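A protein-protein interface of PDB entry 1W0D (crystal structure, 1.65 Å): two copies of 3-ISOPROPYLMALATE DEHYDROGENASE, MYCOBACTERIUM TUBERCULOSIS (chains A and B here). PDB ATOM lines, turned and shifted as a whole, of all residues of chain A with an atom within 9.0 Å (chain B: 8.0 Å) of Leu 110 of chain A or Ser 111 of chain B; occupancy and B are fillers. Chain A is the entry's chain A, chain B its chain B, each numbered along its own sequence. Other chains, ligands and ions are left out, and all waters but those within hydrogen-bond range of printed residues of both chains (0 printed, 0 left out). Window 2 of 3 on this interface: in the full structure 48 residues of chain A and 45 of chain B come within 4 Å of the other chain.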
ATOM      1  N   LEU A 102       7.620   2.831 -25.438  1.00  0.00           N
ATOM      2  CA  LEU A 102       8.680   3.729 -25.852  1.00  0.00           C
ATOM      3  C   LEU A 102       9.840   2.820 -26.248  1.00  0.00           C
ATOM      4  O   LEU A 102      10.414   2.113 -25.418  1.00  0.00           O
ATOM      5  CB  LEU A 102       9.086   4.661 -24.694  1.00  0.00           C
ATOM      6  CG  LEU A 102      10.265   5.565 -25.074  1.00  0.00           C
ATOM      7  CD1 LEU A 102       9.917   6.446 -26.331  1.00  0.00           C
ATOM      8  CD2 LEU A 102      10.588   6.393 -23.833  1.00  0.00           C
ATOM      9  N   VAL A 106      13.410   5.842 -30.449  1.00  0.00           N
ATOM     10  CA  VAL A 106      12.334   6.838 -30.462  1.00  0.00           C
ATOM     11  C   VAL A 106      12.531   7.773 -29.314  1.00  0.00           C
ATOM     12  O   VAL A 106      12.731   7.356 -28.183  1.00  0.00           O
ATOM     13  CB  VAL A 106      10.996   6.133 -30.317  1.00  0.00           C
ATOM     14  CG1 VAL A 106       9.848   7.132 -30.343  1.00  0.00           C
ATOM     15  CG2 VAL A 106      10.865   5.034 -31.376  1.00  0.00           C
ATOM     16  N   ALA A 107      12.471   9.063 -29.600  1.00  0.00           N
ATOM     17  CA  ALA A 107      12.649  10.057 -28.578  1.00  0.00           C
ATOM     18  C   ALA A 107      11.310  10.295 -27.903  1.00  0.00           C
ATOM     19  O   ALA A 107      10.304  10.443 -28.574  1.00  0.00           O
ATOM     20  CB  ALA A 107      13.122  11.357 -29.245  1.00  0.00           C
ATOM     21  N   SER A 108      11.293  10.322 -26.578  1.00  0.00           N
ATOM     22  CA  SER A 108      10.150  10.788 -25.840  1.00  0.00           C
ATOM     23  C   SER A 108      10.318  12.290 -25.630  1.00  0.00           C
ATOM     24  O   SER A 108      11.443  12.819 -25.528  1.00  0.00           O
ATOM     25  CB  SER A 108      10.102  10.069 -24.498  1.00  0.00           C
ATOM     26  OG  SER A 108       9.050  10.568 -23.713  1.00  0.00           O
ATOM     27  N   PRO A 109       9.206  13.005 -25.561  1.00  0.00           N
ATOM     28  CA  PRO A 109       9.212  14.423 -25.199  1.00  0.00           C
ATOM     29  C   PRO A 109       9.430  14.632 -23.702  1.00  0.00           C
ATOM     30  O   PRO A 109       9.658  15.774 -23.239  1.00  0.00           O
ATOM     31  CB  PRO A 109       7.823  14.875 -25.628  1.00  0.00           C
ATOM     32  CG  PRO A 109       6.990  13.677 -25.476  1.00  0.00           C
ATOM     33  CD  PRO A 109       7.860  12.531 -25.930  1.00  0.00           C
ATOM     34  N   LEU A 110       9.339  13.531 -22.952  1.00  0.00           N
ATOM     35  CA  LEU A 110       9.605  13.536 -21.521  1.00  0.00           C
ATOM     36  C   LEU A 110      11.093  13.604 -21.294  1.00  0.00           C
ATOM     37  O   LEU A 110      11.870  13.087 -22.074  1.00  0.00           O
ATOM     38  CB  LEU A 110       9.100  12.247 -20.881  1.00  0.00           C
ATOM     39  CG  LEU A 110       7.592  12.061 -21.085  1.00  0.00           C
ATOM     40  CD1 LEU A 110       7.133  10.872 -20.239  1.00  0.00           C
ATOM     41  CD2 LEU A 110       6.805  13.306 -20.756  1.00  0.00           C
ATOM     42  N   SER A 111      11.464  14.186 -20.164  1.00  0.00           N
ATOM     43  CA  SER A 111      12.843  14.170 -19.717  1.00  0.00           C
ATOM     44  C   SER A 111      13.336  12.730 -19.525  1.00  0.00           C
ATOM     45  O   SER A 111      12.622  11.914 -18.971  1.00  0.00           O
ATOM     46  CB  SER A 111      12.935  14.925 -18.376  1.00  0.00           C
ATOM     47  OG  SER A 111      14.274  15.362 -18.186  1.00  0.00           O
ATOM     48  N   GLY A 112      14.533  12.402 -20.014  1.00  0.00           N
ATOM     49  CA  GLY A 112      15.282  11.261 -19.465  1.00  0.00           C
ATOM     50  C   GLY A 112      14.998   9.759 -19.690  1.00  0.00           C
ATOM     51  O   GLY A 112      15.333   8.900 -18.810  1.00  0.00           O
ATOM     52  N   ASN A 113      14.439   9.451 -20.843  1.00  0.00           N
ATOM     53  CA  ASN A 113      14.223   8.091 -21.366  1.00  0.00           C
ATOM     54  C   ASN A 113      13.617   7.017 -20.448  1.00  0.00           C
ATOM     55  O   ASN A 113      14.179   5.911 -20.344  1.00  0.00           O
ATOM     56  CB  ASN A 113      15.526   7.542 -21.997  1.00  0.00           C
ATOM     57  CG  ASN A 113      15.241   6.403 -22.943  1.00  0.00           C
ATOM     58  OD1 ASN A 113      14.169   6.390 -23.520  1.00  0.00           O
ATOM     59  ND2 ASN A 113      16.145   5.451 -23.075  1.00  0.00           N
ATOM     60  N   PRO A 114      12.485   7.291 -19.801  1.00  0.00           N
ATOM     61  CA  PRO A 114      11.914   6.274 -18.906  1.00  0.00           C
ATOM     62  C   PRO A 114      11.454   5.067 -19.722  1.00  0.00           C
ATOM     63  O   PRO A 114      11.110   5.135 -20.921  1.00  0.00           O
ATOM     64  CB  PRO A 114      10.751   6.996 -18.221  1.00  0.00           C
ATOM     65  CG  PRO A 114      10.389   8.086 -19.222  1.00  0.00           C
ATOM     66  CD  PRO A 114      11.688   8.530 -19.830  1.00  0.00           C
ATOM     67  N   GLY A 115      11.464   3.921 -19.069  1.00  0.00           N
ATOM     68  CA  GLY A 115      10.867   2.762 -19.672  1.00  0.00           C
ATOM     69  C   GLY A 115       9.387   3.014 -19.630  1.00  0.00           C
ATOM     70  O   GLY A 115       8.846   3.385 -18.608  1.00  0.00           O
ATOM     71  N   ILE A 116       8.730   2.865 -20.756  1.00  0.00           N
ATOM     72  CA  ILE A 116       7.291   3.008 -20.772  1.00  0.00           C
ATOM     73  C   ILE A 116       6.771   1.855 -21.570  1.00  0.00           C
ATOM     74  O   ILE A 116       7.181   1.679 -22.680  1.00  0.00           O
ATOM     75  CB  ILE A 116       6.889   4.264 -21.560  1.00  0.00           C
ATOM     76  CG1 ILE A 116       7.622   5.505 -21.050  1.00  0.00           C
ATOM     77  CG2 ILE A 116       5.332   4.370 -21.565  1.00  0.00           C
ATOM     78  CD1 ILE A 116       7.211   6.805 -21.749  1.00  0.00           C
ATOM     79  N   PHE A 118       2.946   0.398 -21.624  1.00  0.00           N
ATOM     80  CA  PHE A 118       1.588   0.157 -21.137  1.00  0.00           C
ATOM     81  C   PHE A 118       0.629   0.022 -22.260  1.00  0.00           C
ATOM     82  O   PHE A 118       0.981   0.229 -23.419  1.00  0.00           O
ATOM     83  CB  PHE A 118       1.140   1.173 -20.104  1.00  0.00           C
ATOM     84  CG  PHE A 118       1.057   2.597 -20.591  1.00  0.00           C
ATOM     85  CD1 PHE A 118      -0.142   3.075 -21.101  1.00  0.00           C
ATOM     86  CD2 PHE A 118       2.107   3.469 -20.444  1.00  0.00           C
ATOM     87  CE1 PHE A 118      -0.265   4.379 -21.512  1.00  0.00           C
ATOM     88  CE2 PHE A 118       1.989   4.810 -20.866  1.00  0.00           C
ATOM     89  CZ  PHE A 118       0.809   5.259 -21.397  1.00  0.00           C
ATOM     90  N   THR A 215      -3.187  11.842 -16.246  1.00  0.00           N
ATOM     91  CA  THR A 215      -2.505  12.675 -17.202  1.00  0.00           C
ATOM     92  C   THR A 215      -1.147  13.116 -16.661  1.00  0.00           C
ATOM     93  O   THR A 215      -0.123  12.951 -17.343  1.00  0.00           O
ATOM     94  CB  THR A 215      -3.422  13.894 -17.526  1.00  0.00           C
ATOM     95  OG1 THR A 215      -4.424  13.481 -18.495  1.00  0.00           O
ATOM     96  CG2 THR A 215      -2.690  14.937 -18.214  1.00  0.00           C
ATOM     97  N   ILE A 216      -1.154  13.664 -15.432  1.00  0.00           N
ATOM     98  CA  ILE A 216       0.096  13.987 -14.731  1.00  0.00           C
ATOM     99  C   ILE A 216       1.035  12.791 -14.662  1.00  0.00           C
ATOM    100  O   ILE A 216       2.201  12.913 -15.009  1.00  0.00           O
ATOM    101  CB  ILE A 216      -0.181  14.564 -13.315  1.00  0.00           C
ATOM    102  CG1 ILE A 216      -0.883  15.909 -13.443  1.00  0.00           C
ATOM    103  CG2 ILE A 216       1.106  14.713 -12.535  1.00  0.00           C
ATOM    104  CD1 ILE A 216      -1.412  16.480 -12.176  1.00  0.00           C
ATOM    105  N   HIS A 217       0.552  11.639 -14.243  1.00  0.00           N
ATOM    106  CA  HIS A 217       1.453  10.498 -14.097  1.00  0.00           C
ATOM    107  C   HIS A 217       1.958   9.972 -15.419  1.00  0.00           C
ATOM    108  O   HIS A 217       3.074   9.459 -15.497  1.00  0.00           O
ATOM    109  CB  HIS A 217       0.798   9.407 -13.275  1.00  0.00           C
ATOM    110  CG  HIS A 217       0.860   9.683 -11.804  1.00  0.00           C
ATOM    111  ND1 HIS A 217      -0.169   9.390 -10.945  1.00  0.00           N
ATOM    112  CD2 HIS A 217       1.819  10.280 -11.053  1.00  0.00           C
ATOM    113  CE1 HIS A 217       0.151   9.777  -9.724  1.00  0.00           C
ATOM    114  NE2 HIS A 217       1.357  10.314  -9.760  1.00  0.00           N
ATOM    115  N   MET A 218       1.192  10.145 -16.487  1.00  0.00           N
ATOM    116  CA  MET A 218       1.718   9.798 -17.803  1.00  0.00           C
ATOM    117  C   MET A 218       2.986  10.587 -18.167  1.00  0.00           C
ATOM    118  O   MET A 218       3.735  10.136 -19.028  1.00  0.00           O
ATOM    119  CB  MET A 218       0.669   9.991 -18.905  1.00  0.00           C
ATOM    120  CG  MET A 218       0.631   8.845 -19.939  1.00  0.00           C
ATOM    121  SD  MET A 218      -1.009   8.715 -20.751  1.00  0.00           S
ATOM    122  CE  MET A 218      -2.055   8.376 -19.391  1.00  0.00           C
ATOM    123  N   ILE A 219       3.111  11.801 -17.611  1.00  0.00           N
ATOM    124  CA  ILE A 219       4.209  12.750 -17.865  1.00  0.00           C
ATOM    125  C   ILE A 219       5.333  12.575 -16.847  1.00  0.00           C
ATOM    126  O   ILE A 219       6.465  12.789 -17.168  1.00  0.00           O
ATOM    127  CB  ILE A 219       3.655  14.227 -17.830  1.00  0.00           C
ATOM    128  CG1 ILE A 219       2.549  14.388 -18.871  1.00  0.00           C
ATOM    129  CG2 ILE A 219       4.696  15.253 -18.168  1.00  0.00           C
ATOM    130  CD1 ILE A 219       2.909  13.846 -20.211  1.00  0.00           C
ATOM    131  N   THR A 220       5.009  12.239 -15.608  1.00  0.00           N
ATOM    132  CA  THR A 220       6.000  12.219 -14.556  1.00  0.00           C
ATOM    133  C   THR A 220       6.423  10.820 -14.184  1.00  0.00           C
ATOM    134  O   THR A 220       7.526  10.644 -13.689  1.00  0.00           O
ATOM    135  CB  THR A 220       5.548  12.936 -13.290  1.00  0.00           C
ATOM    136  OG1 THR A 220       4.389  12.288 -12.747  1.00  0.00           O
ATOM    137  CG2 THR A 220       5.105  14.355 -13.584  1.00  0.00           C
ATOM    138  N   ASP A 221       5.592   9.829 -14.487  1.00  0.00           N
ATOM    139  CA  ASP A 221       5.804   8.483 -14.004  1.00  0.00           C
ATOM    140  C   ASP A 221       5.110   7.435 -14.895  1.00  0.00           C
ATOM    141  O   ASP A 221       4.411   6.545 -14.407  1.00  0.00           O
ATOM    142  CB  ASP A 221       5.278   8.446 -12.568  1.00  0.00           C
ATOM    143  CG  ASP A 221       5.609   7.194 -11.876  1.00  0.00           C
ATOM    144  OD1 ASP A 221       6.694   6.628 -12.143  1.00  0.00           O
ATOM    145  OD2 ASP A 221       4.827   6.732 -11.010  1.00  0.00           O
ATOM    146  N   PRO A 222       5.281   7.528 -16.216  1.00  0.00           N
ATOM    147  CA  PRO A 222       4.553   6.634 -17.119  1.00  0.00           C
ATOM    148  C   PRO A 222       4.900   5.183 -16.919  1.00  0.00           C
ATOM    149  O   PRO A 222       4.162   4.303 -17.363  1.00  0.00           O
ATOM    150  CB  PRO A 222       4.974   7.114 -18.506  1.00  0.00           C
ATOM    151  CG  PRO A 222       6.314   7.726 -18.263  1.00  0.00           C
ATOM    152  CD  PRO A 222       6.124   8.476 -16.952  1.00  0.00           C
ATOM    153  N   GLY A 223       6.042   4.896 -16.300  1.00  0.00           N
ATOM    154  CA  GLY A 223       6.343   3.507 -16.022  1.00  0.00           C
ATOM    155  C   GLY A 223       5.421   2.872 -14.977  1.00  0.00           C
ATOM    156  O   GLY A 223       5.538   1.657 -14.751  1.00  0.00           O
ATOM    157  N   LEU A 241      -2.302  11.125 -25.392  1.00  0.00           N
ATOM    158  CA  LEU A 241      -1.217  11.507 -24.510  1.00  0.00           C
ATOM    159  C   LEU A 241      -0.189  10.378 -24.434  1.00  0.00           C
ATOM    160  O   LEU A 241       1.024  10.666 -24.499  1.00  0.00           O
ATOM    161  CB  LEU A 241      -1.748  11.872 -23.121  1.00  0.00           C
ATOM    162  CG  LEU A 241      -0.683  12.465 -22.209  1.00  0.00           C
ATOM    163  CD1 LEU A 241      -0.180  13.858 -22.724  1.00  0.00           C
ATOM    164  CD2 LEU A 241      -1.275  12.529 -20.778  1.00  0.00           C
ATOM    165  N   ALA A 242      -0.648   9.126 -24.409  1.00  0.00           N
ATOM    166  CA  ALA A 242       0.195   7.948 -24.348  1.00  0.00           C
ATOM    167  C   ALA A 242       1.103   7.932 -25.567  1.00  0.00           C
ATOM    168  O   ALA A 242       2.306   7.661 -25.479  1.00  0.00           O
ATOM    169  CB  ALA A 242      -0.646   6.678 -24.324  1.00  0.00           C
ATOM    170  N   ALA A 243       0.515   8.222 -26.724  1.00  0.00           N
ATOM    171  CA  ALA A 243       1.266   8.111 -27.972  1.00  0.00           C
ATOM    172  C   ALA A 243       2.302   9.192 -27.906  1.00  0.00           C
ATOM    173  O   ALA A 243       3.464   8.960 -28.245  1.00  0.00           O
ATOM    174  CB  ALA A 243       0.359   8.300 -29.187  1.00  0.00           C
ATOM    175  N   ALA A 244       1.914  10.378 -27.436  1.00  0.00           N
ATOM    176  CA  ALA A 244       2.903  11.432 -27.403  1.00  0.00           C
ATOM    177  C   ALA A 244       4.077  11.075 -26.512  1.00  0.00           C
ATOM    178  O   ALA A 244       5.228  11.319 -26.893  1.00  0.00           O
ATOM    179  CB  ALA A 244       2.293  12.732 -26.941  1.00  0.00           C
ATOM    180  N   VAL A 245       3.826  10.478 -25.342  1.00  0.00           N
ATOM    181  CA  VAL A 245       4.966  10.298 -24.465  1.00  0.00           C
ATOM    182  C   VAL A 245       5.865   9.160 -25.025  1.00  0.00           C
ATOM    183  O   VAL A 245       7.050   9.093 -24.705  1.00  0.00           O
ATOM    184  CB  VAL A 245       4.629  10.062 -22.972  1.00  0.00           C
ATOM    185  CG1 VAL A 245       3.846  11.229 -22.366  1.00  0.00           C
ATOM    186  CG2 VAL A 245       3.879   8.784 -22.756  1.00  0.00           C
ATOM    187  N   CYS A 246       5.289   8.344 -25.915  1.00  0.00           N
ATOM    188  CA  CYS A 246       5.967   7.228 -26.567  1.00  0.00           C
ATOM    189  C   CYS A 246       6.516   7.617 -27.918  1.00  0.00           C
ATOM    190  O   CYS A 246       6.917   6.755 -28.707  1.00  0.00           O
ATOM    191  CB  CYS A 246       5.005   6.027 -26.632  1.00  0.00           C
ATOM    192  SG  CYS A 246       4.864   5.370 -24.969  1.00  0.00           S
ATOM    193  N   GLY A 247       6.572   8.929 -28.169  1.00  0.00           N
ATOM    194  CA  GLY A 247       7.180   9.437 -29.385  1.00  0.00           C
ATOM    195  C   GLY A 247       6.264   9.865 -30.511  1.00  0.00           C
ATOM    196  O   GLY A 247       6.753  10.205 -31.625  1.00  0.00           O
ATOM    197  N   LEU B 102       6.497  27.990 -16.909  1.00  0.00           N
ATOM    198  CA  LEU B 102       7.662  27.285 -16.441  1.00  0.00           C
ATOM    199  C   LEU B 102       8.685  28.362 -16.151  1.00  0.00           C
ATOM    200  O   LEU B 102       9.112  29.091 -17.049  1.00  0.00           O
ATOM    201  CB  LEU B 102       8.173  26.305 -17.502  1.00  0.00           C
ATOM    202  CG  LEU B 102       9.393  25.504 -17.101  1.00  0.00           C
ATOM    203  CD1 LEU B 102       9.104  24.527 -15.954  1.00  0.00           C
ATOM    204  CD2 LEU B 102       9.929  24.769 -18.318  1.00  0.00           C
ATOM    205  N   SER B 108      11.057  20.980 -15.507  1.00  0.00           N
ATOM    206  CA  SER B 108       9.891  20.459 -16.185  1.00  0.00           C
ATOM    207  C   SER B 108      10.147  18.951 -16.376  1.00  0.00           C
ATOM    208  O   SER B 108      11.284  18.563 -16.644  1.00  0.00           O
ATOM    209  CB  SER B 108       9.784  21.168 -17.528  1.00  0.00           C
ATOM    210  OG  SER B 108       8.823  20.548 -18.359  1.00  0.00           O
ATOM    211  N   PRO B 109       9.097  18.133 -16.247  1.00  0.00           N
ATOM    212  CA  PRO B 109       9.141  16.704 -16.598  1.00  0.00           C
ATOM    213  C   PRO B 109       9.327  16.508 -18.110  1.00  0.00           C
ATOM    214  O   PRO B 109       9.545  15.380 -18.543  1.00  0.00           O
ATOM    215  CB  PRO B 109       7.769  16.212 -16.183  1.00  0.00           C
ATOM    216  CG  PRO B 109       6.904  17.432 -16.346  1.00  0.00           C
ATOM    217  CD  PRO B 109       7.773  18.517 -15.742  1.00  0.00           C
ATOM    218  N   LEU B 110       9.251  17.595 -18.874  1.00  0.00           N
ATOM    219  CA  LEU B 110       9.499  17.571 -20.312  1.00  0.00           C
ATOM    220  C   LEU B 110      10.968  17.743 -20.570  1.00  0.00           C
ATOM    221  O   LEU B 110      11.664  18.408 -19.793  1.00  0.00           O
ATOM    222  CB  LEU B 110       8.773  18.725 -21.018  1.00  0.00           C
ATOM    223  CG  LEU B 110       7.238  18.737 -20.846  1.00  0.00           C
ATOM    224  CD1 LEU B 110       6.610  19.749 -21.749  1.00  0.00           C
ATOM    225  CD2 LEU B 110       6.600  17.319 -21.063  1.00  0.00           C
ATOM    226  N   SER B 111      11.414  17.181 -21.695  1.00  0.00           N
ATOM    227  CA  SER B 111      12.801  17.252 -22.156  1.00  0.00           C
ATOM    228  C   SER B 111      13.162  18.644 -22.640  1.00  0.00           C
ATOM    229  O   SER B 111      12.362  19.310 -23.321  1.00  0.00           O
ATOM    230  CB  SER B 111      13.033  16.252 -23.295  1.00  0.00           C
ATOM    231  OG  SER B 111      14.320  16.443 -23.871  1.00  0.00           O
ATOM    232  N   GLY B 112      14.374  19.072 -22.295  1.00  0.00           N
ATOM    233  CA  GLY B 112      14.956  20.260 -22.879  1.00  0.00           C
ATOM    234  C   GLY B 112      14.425  21.605 -22.431  1.00  0.00           C
ATOM    235  O   GLY B 112      14.430  22.553 -23.211  1.00  0.00           O
ATOM    236  N   ASN B 113      14.004  21.701 -21.172  1.00  0.00           N
ATOM    237  CA  ASN B 113      13.412  22.940 -20.635  1.00  0.00           C
ATOM    238  C   ASN B 113      12.794  23.951 -21.634  1.00  0.00           C
ATOM    239  O   ASN B 113      13.339  25.034 -21.859  1.00  0.00           O
ATOM    240  CB  ASN B 113      14.350  23.643 -19.634  1.00  0.00           C
ATOM    241  CG  ASN B 113      13.601  24.084 -18.375  1.00  0.00           C
ATOM    242  OD1 ASN B 113      13.081  23.235 -17.610  1.00  0.00           O
ATOM    243  ND2 ASN B 113      13.489  25.400 -18.179  1.00  0.00           N
ATOM    244  N   PRO B 114      11.638  23.595 -22.205  1.00  0.00           N
ATOM    245  CA  PRO B 114      10.964  24.423 -23.220  1.00  0.00           C
ATOM    246  C   PRO B 114      10.355  25.691 -22.630  1.00  0.00           C
ATOM    247  O   PRO B 114      10.101  25.716 -21.418  1.00  0.00           O
ATOM    248  CB  PRO B 114       9.849  23.520 -23.701  1.00  0.00           C
ATOM    249  CG  PRO B 114       9.560  22.675 -22.524  1.00  0.00           C
ATOM    250  CD  PRO B 114      10.886  22.366 -21.914  1.00  0.00           C
ATOM    251  N   GLY B 115      10.135  26.714 -23.454  1.00  0.00           N
ATOM    252  CA  GLY B 115       9.539  27.943 -22.974  1.00  0.00           C
ATOM    253  C   GLY B 115       8.071  27.617 -22.828  1.00  0.00           C
ATOM    254  O   GLY B 115       7.499  27.084 -23.764  1.00  0.00           O
ATOM    255  N   ILE B 219       2.636  18.633 -24.304  1.00  0.00           N
ATOM    256  CA  ILE B 219       3.866  17.939 -23.942  1.00  0.00           C
ATOM    257  C   ILE B 219       4.928  18.028 -25.026  1.00  0.00           C
ATOM    258  O   ILE B 219       6.130  17.950 -24.744  1.00  0.00           O
ATOM    259  CB  ILE B 219       3.564  16.490 -23.543  1.00  0.00           C
ATOM    260  CG1 ILE B 219       3.208  15.658 -24.750  1.00  0.00           C
ATOM    261  CG2 ILE B 219       2.477  16.435 -22.474  1.00  0.00           C
ATOM    262  CD1 ILE B 219       3.333  14.169 -24.460  1.00  0.00           C
ATOM    263  N   THR B 220       4.509  18.192 -26.274  1.00  0.00           N
ATOM    264  CA  THR B 220       5.508  18.250 -27.339  1.00  0.00           C
ATOM    265  C   THR B 220       5.784  19.666 -27.754  1.00  0.00           C
ATOM    266  O   THR B 220       6.866  19.968 -28.224  1.00  0.00           O
ATOM    267  CB  THR B 220       5.052  17.491 -28.570  1.00  0.00           C
ATOM    268  OG1 THR B 220       3.814  18.048 -29.020  1.00  0.00           O
ATOM    269  CG2 THR B 220       4.758  15.995 -28.230  1.00  0.00           C
ATOM    270  N   PRO B 222       4.573  22.925 -25.908  1.00  0.00           N
ATOM    271  CA  PRO B 222       3.764  23.749 -25.011  1.00  0.00           C
ATOM    272  C   PRO B 222       3.934  25.213 -25.274  1.00  0.00           C
ATOM    273  O   PRO B 222       3.063  26.001 -24.908  1.00  0.00           O
ATOM    274  CB  PRO B 222       4.255  23.358 -23.612  1.00  0.00           C
ATOM    275  CG  PRO B 222       5.601  22.786 -23.831  1.00  0.00           C
ATOM    276  CD  PRO B 222       5.587  22.133 -25.182  1.00  0.00           C
ATOM    277  N   LEU B 241      -2.528  18.869 -16.473  1.00  0.00           N
ATOM    278  CA  LEU B 241      -1.413  18.586 -17.370  1.00  0.00           C
ATOM    279  C   LEU B 241      -0.471  19.794 -17.438  1.00  0.00           C
ATOM    280  O   LEU B 241       0.773  19.649 -17.359  1.00  0.00           O
ATOM    281  CB  LEU B 241      -1.926  18.253 -18.771  1.00  0.00           C
ATOM    282  CG  LEU B 241      -0.923  17.888 -19.878  1.00  0.00           C
ATOM    283  CD1 LEU B 241       0.225  16.951 -19.416  1.00  0.00           C
ATOM    284  CD2 LEU B 241      -1.651  17.348 -21.104  1.00  0.00           C
ATOM    285  N   VAL B 245       3.630  19.984 -16.581  1.00  0.00           N
ATOM    286  CA  VAL B 245       4.726  20.315 -17.461  1.00  0.00           C
ATOM    287  C   VAL B 245       5.432  21.575 -16.957  1.00  0.00           C
ATOM    288  O   VAL B 245       6.584  21.779 -17.262  1.00  0.00           O
ATOM    289  CB  VAL B 245       4.278  20.506 -18.952  1.00  0.00           C
ATOM    290  CG1 VAL B 245       3.557  19.266 -19.449  1.00  0.00           C
ATOM    291  CG2 VAL B 245       3.444  21.787 -19.156  1.00  0.00           C
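Of the 29 printed residues of chain A, 8 touch a printed residue of chain B.
Hydrophobic or aromatic side chains of chain A within 4 Å of the printed part of chain B: Pro 109, Leu 110, Ile 219, Leu 241, Ala 244 and Val 245.
Along chain A the printed residues that touch a printed residue of chain B span positions 109 to 245.
Of the 14 printed residues of chain B, 5 touch a printed residue of chain A.
Hydrophobic or aromatic side chains of chain B that line the printed part of chain A: Pro 109, Leu 110, Ile 219 and Leu 241.
Among the printed residues, no Asp or Glu carboxylate lies within 4 Å of a Lys or Arg side-chain nitrogen of the other chain.
Among the printed residues, pairs that only touch across the chains: Pro 109 of chain A with Leu 110 of chain B (3.4 Å), Pro 109 of chain A with Ile 219 of chain B (3.6 Å), Leu 110 of chain A with Pro 109 of chain B (3.5 Å), Leu 110 of chain A with Ser 111 of chain B (3.6 Å), Ser 111 of chain A with Leu 110 of chain B (3.6 Å), Thr 215 of chain A with Leu 241 of chain B (3.4 Å), Ile 219 of chain A with Pro 109 of chain B (3.6 Å), Ile 219 of chain A with Ile 219 of chain B (3.5 Å), Ile 219 of chain A with Leu 241 of chain B (3.5 Å), Leu 241 of chain A with Ile 219 of chain B (3.7 Å), Ala 244 of chain A with Ile 219 of chain B (3.0 Å) and Val 245 of chain A with Ile 219 of chain B (3.6 Å).
Pro 109 of chain A touches Ile 219 of chain B, and with the chains exchanged Ile 219 of chain A touches Pro 109 of chain B.
Leu 110 of chain A touches Ser 111 of chain B, and with the chains exchanged Ser 111 of chain A touches Leu 110 of chain B.
Ser 111 of chain A touches its own counterpart, Ser 111 of chain B.
Val 245 of chain A touches Ile 219 of chain B, but with the chains exchanged Ile 219 of chain A does not touch Val 245 of chain B (4.4 Å).
14 positions are printed for both chains.
Of the 15 pairs that touch across the chains among the printed residues, 12 have their exchanged pair printed and touching as well.
Leu 110 of chain A touches two residues of chain B.
Printed residues of chain A within 4 Å of Ser 111 of chain B: Pro 109 (2.7 Å), Leu 110 (3.6 Å) and Ser 111 (3.4 Å).
Pro 109 of chain A touches just these residues of chain B: Leu 110, Ser 111 and Ile 219.
No residue of chain A comes within 4 Å of Gly 112 of chain B.
Of the printed residues of chain B, Leu 241 of chain A touches Ile 219 (3.7 Å).
Of the printed residues of chain B, Val 245 of chain A touches Ile 219 (3.6 Å).
Printed residues of chain A within 4 Å of Leu 241 of chain B: Thr 215 and Ile 219.
Gly 223 of chain A touches none of the printed residues of chain B.
Leu 102 of chain A touches none of the printed residues of chain B.
The nearest residue of chain A that does not touch Ser 111 of chain B is Ser 108 of chain A (4.4 Å).
The nearest printed residue of chain A that does not touch Leu 241 of chain B is Leu 241 of chain A (4.1 Å).
N of Leu 110 of chain A lies within hydrogen-bond range of OG of Ser 108 of chain A (3.1 Å).
OG of Ser 108 of chain A lies within hydrogen-bond range of O of Val 245 of chain A (2.7 Å).
N of Leu 110 of chain B sits close to OG of Ser 108 of chain B (3.0 Å).
The backbone NH of Ser 111 of chain B sits close to the backbone NH of Ser 111 of chain A.
The backbone carbonyl oxygen (O) of Pro 109 of chain A sits at hydrogen-bond distance from the backbone NH (N) of Ser 111 of chain B.
N of Ser 111 of chain A is in hydrogen-bond range of O of Pro 109 of chain B (2.8 Å).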
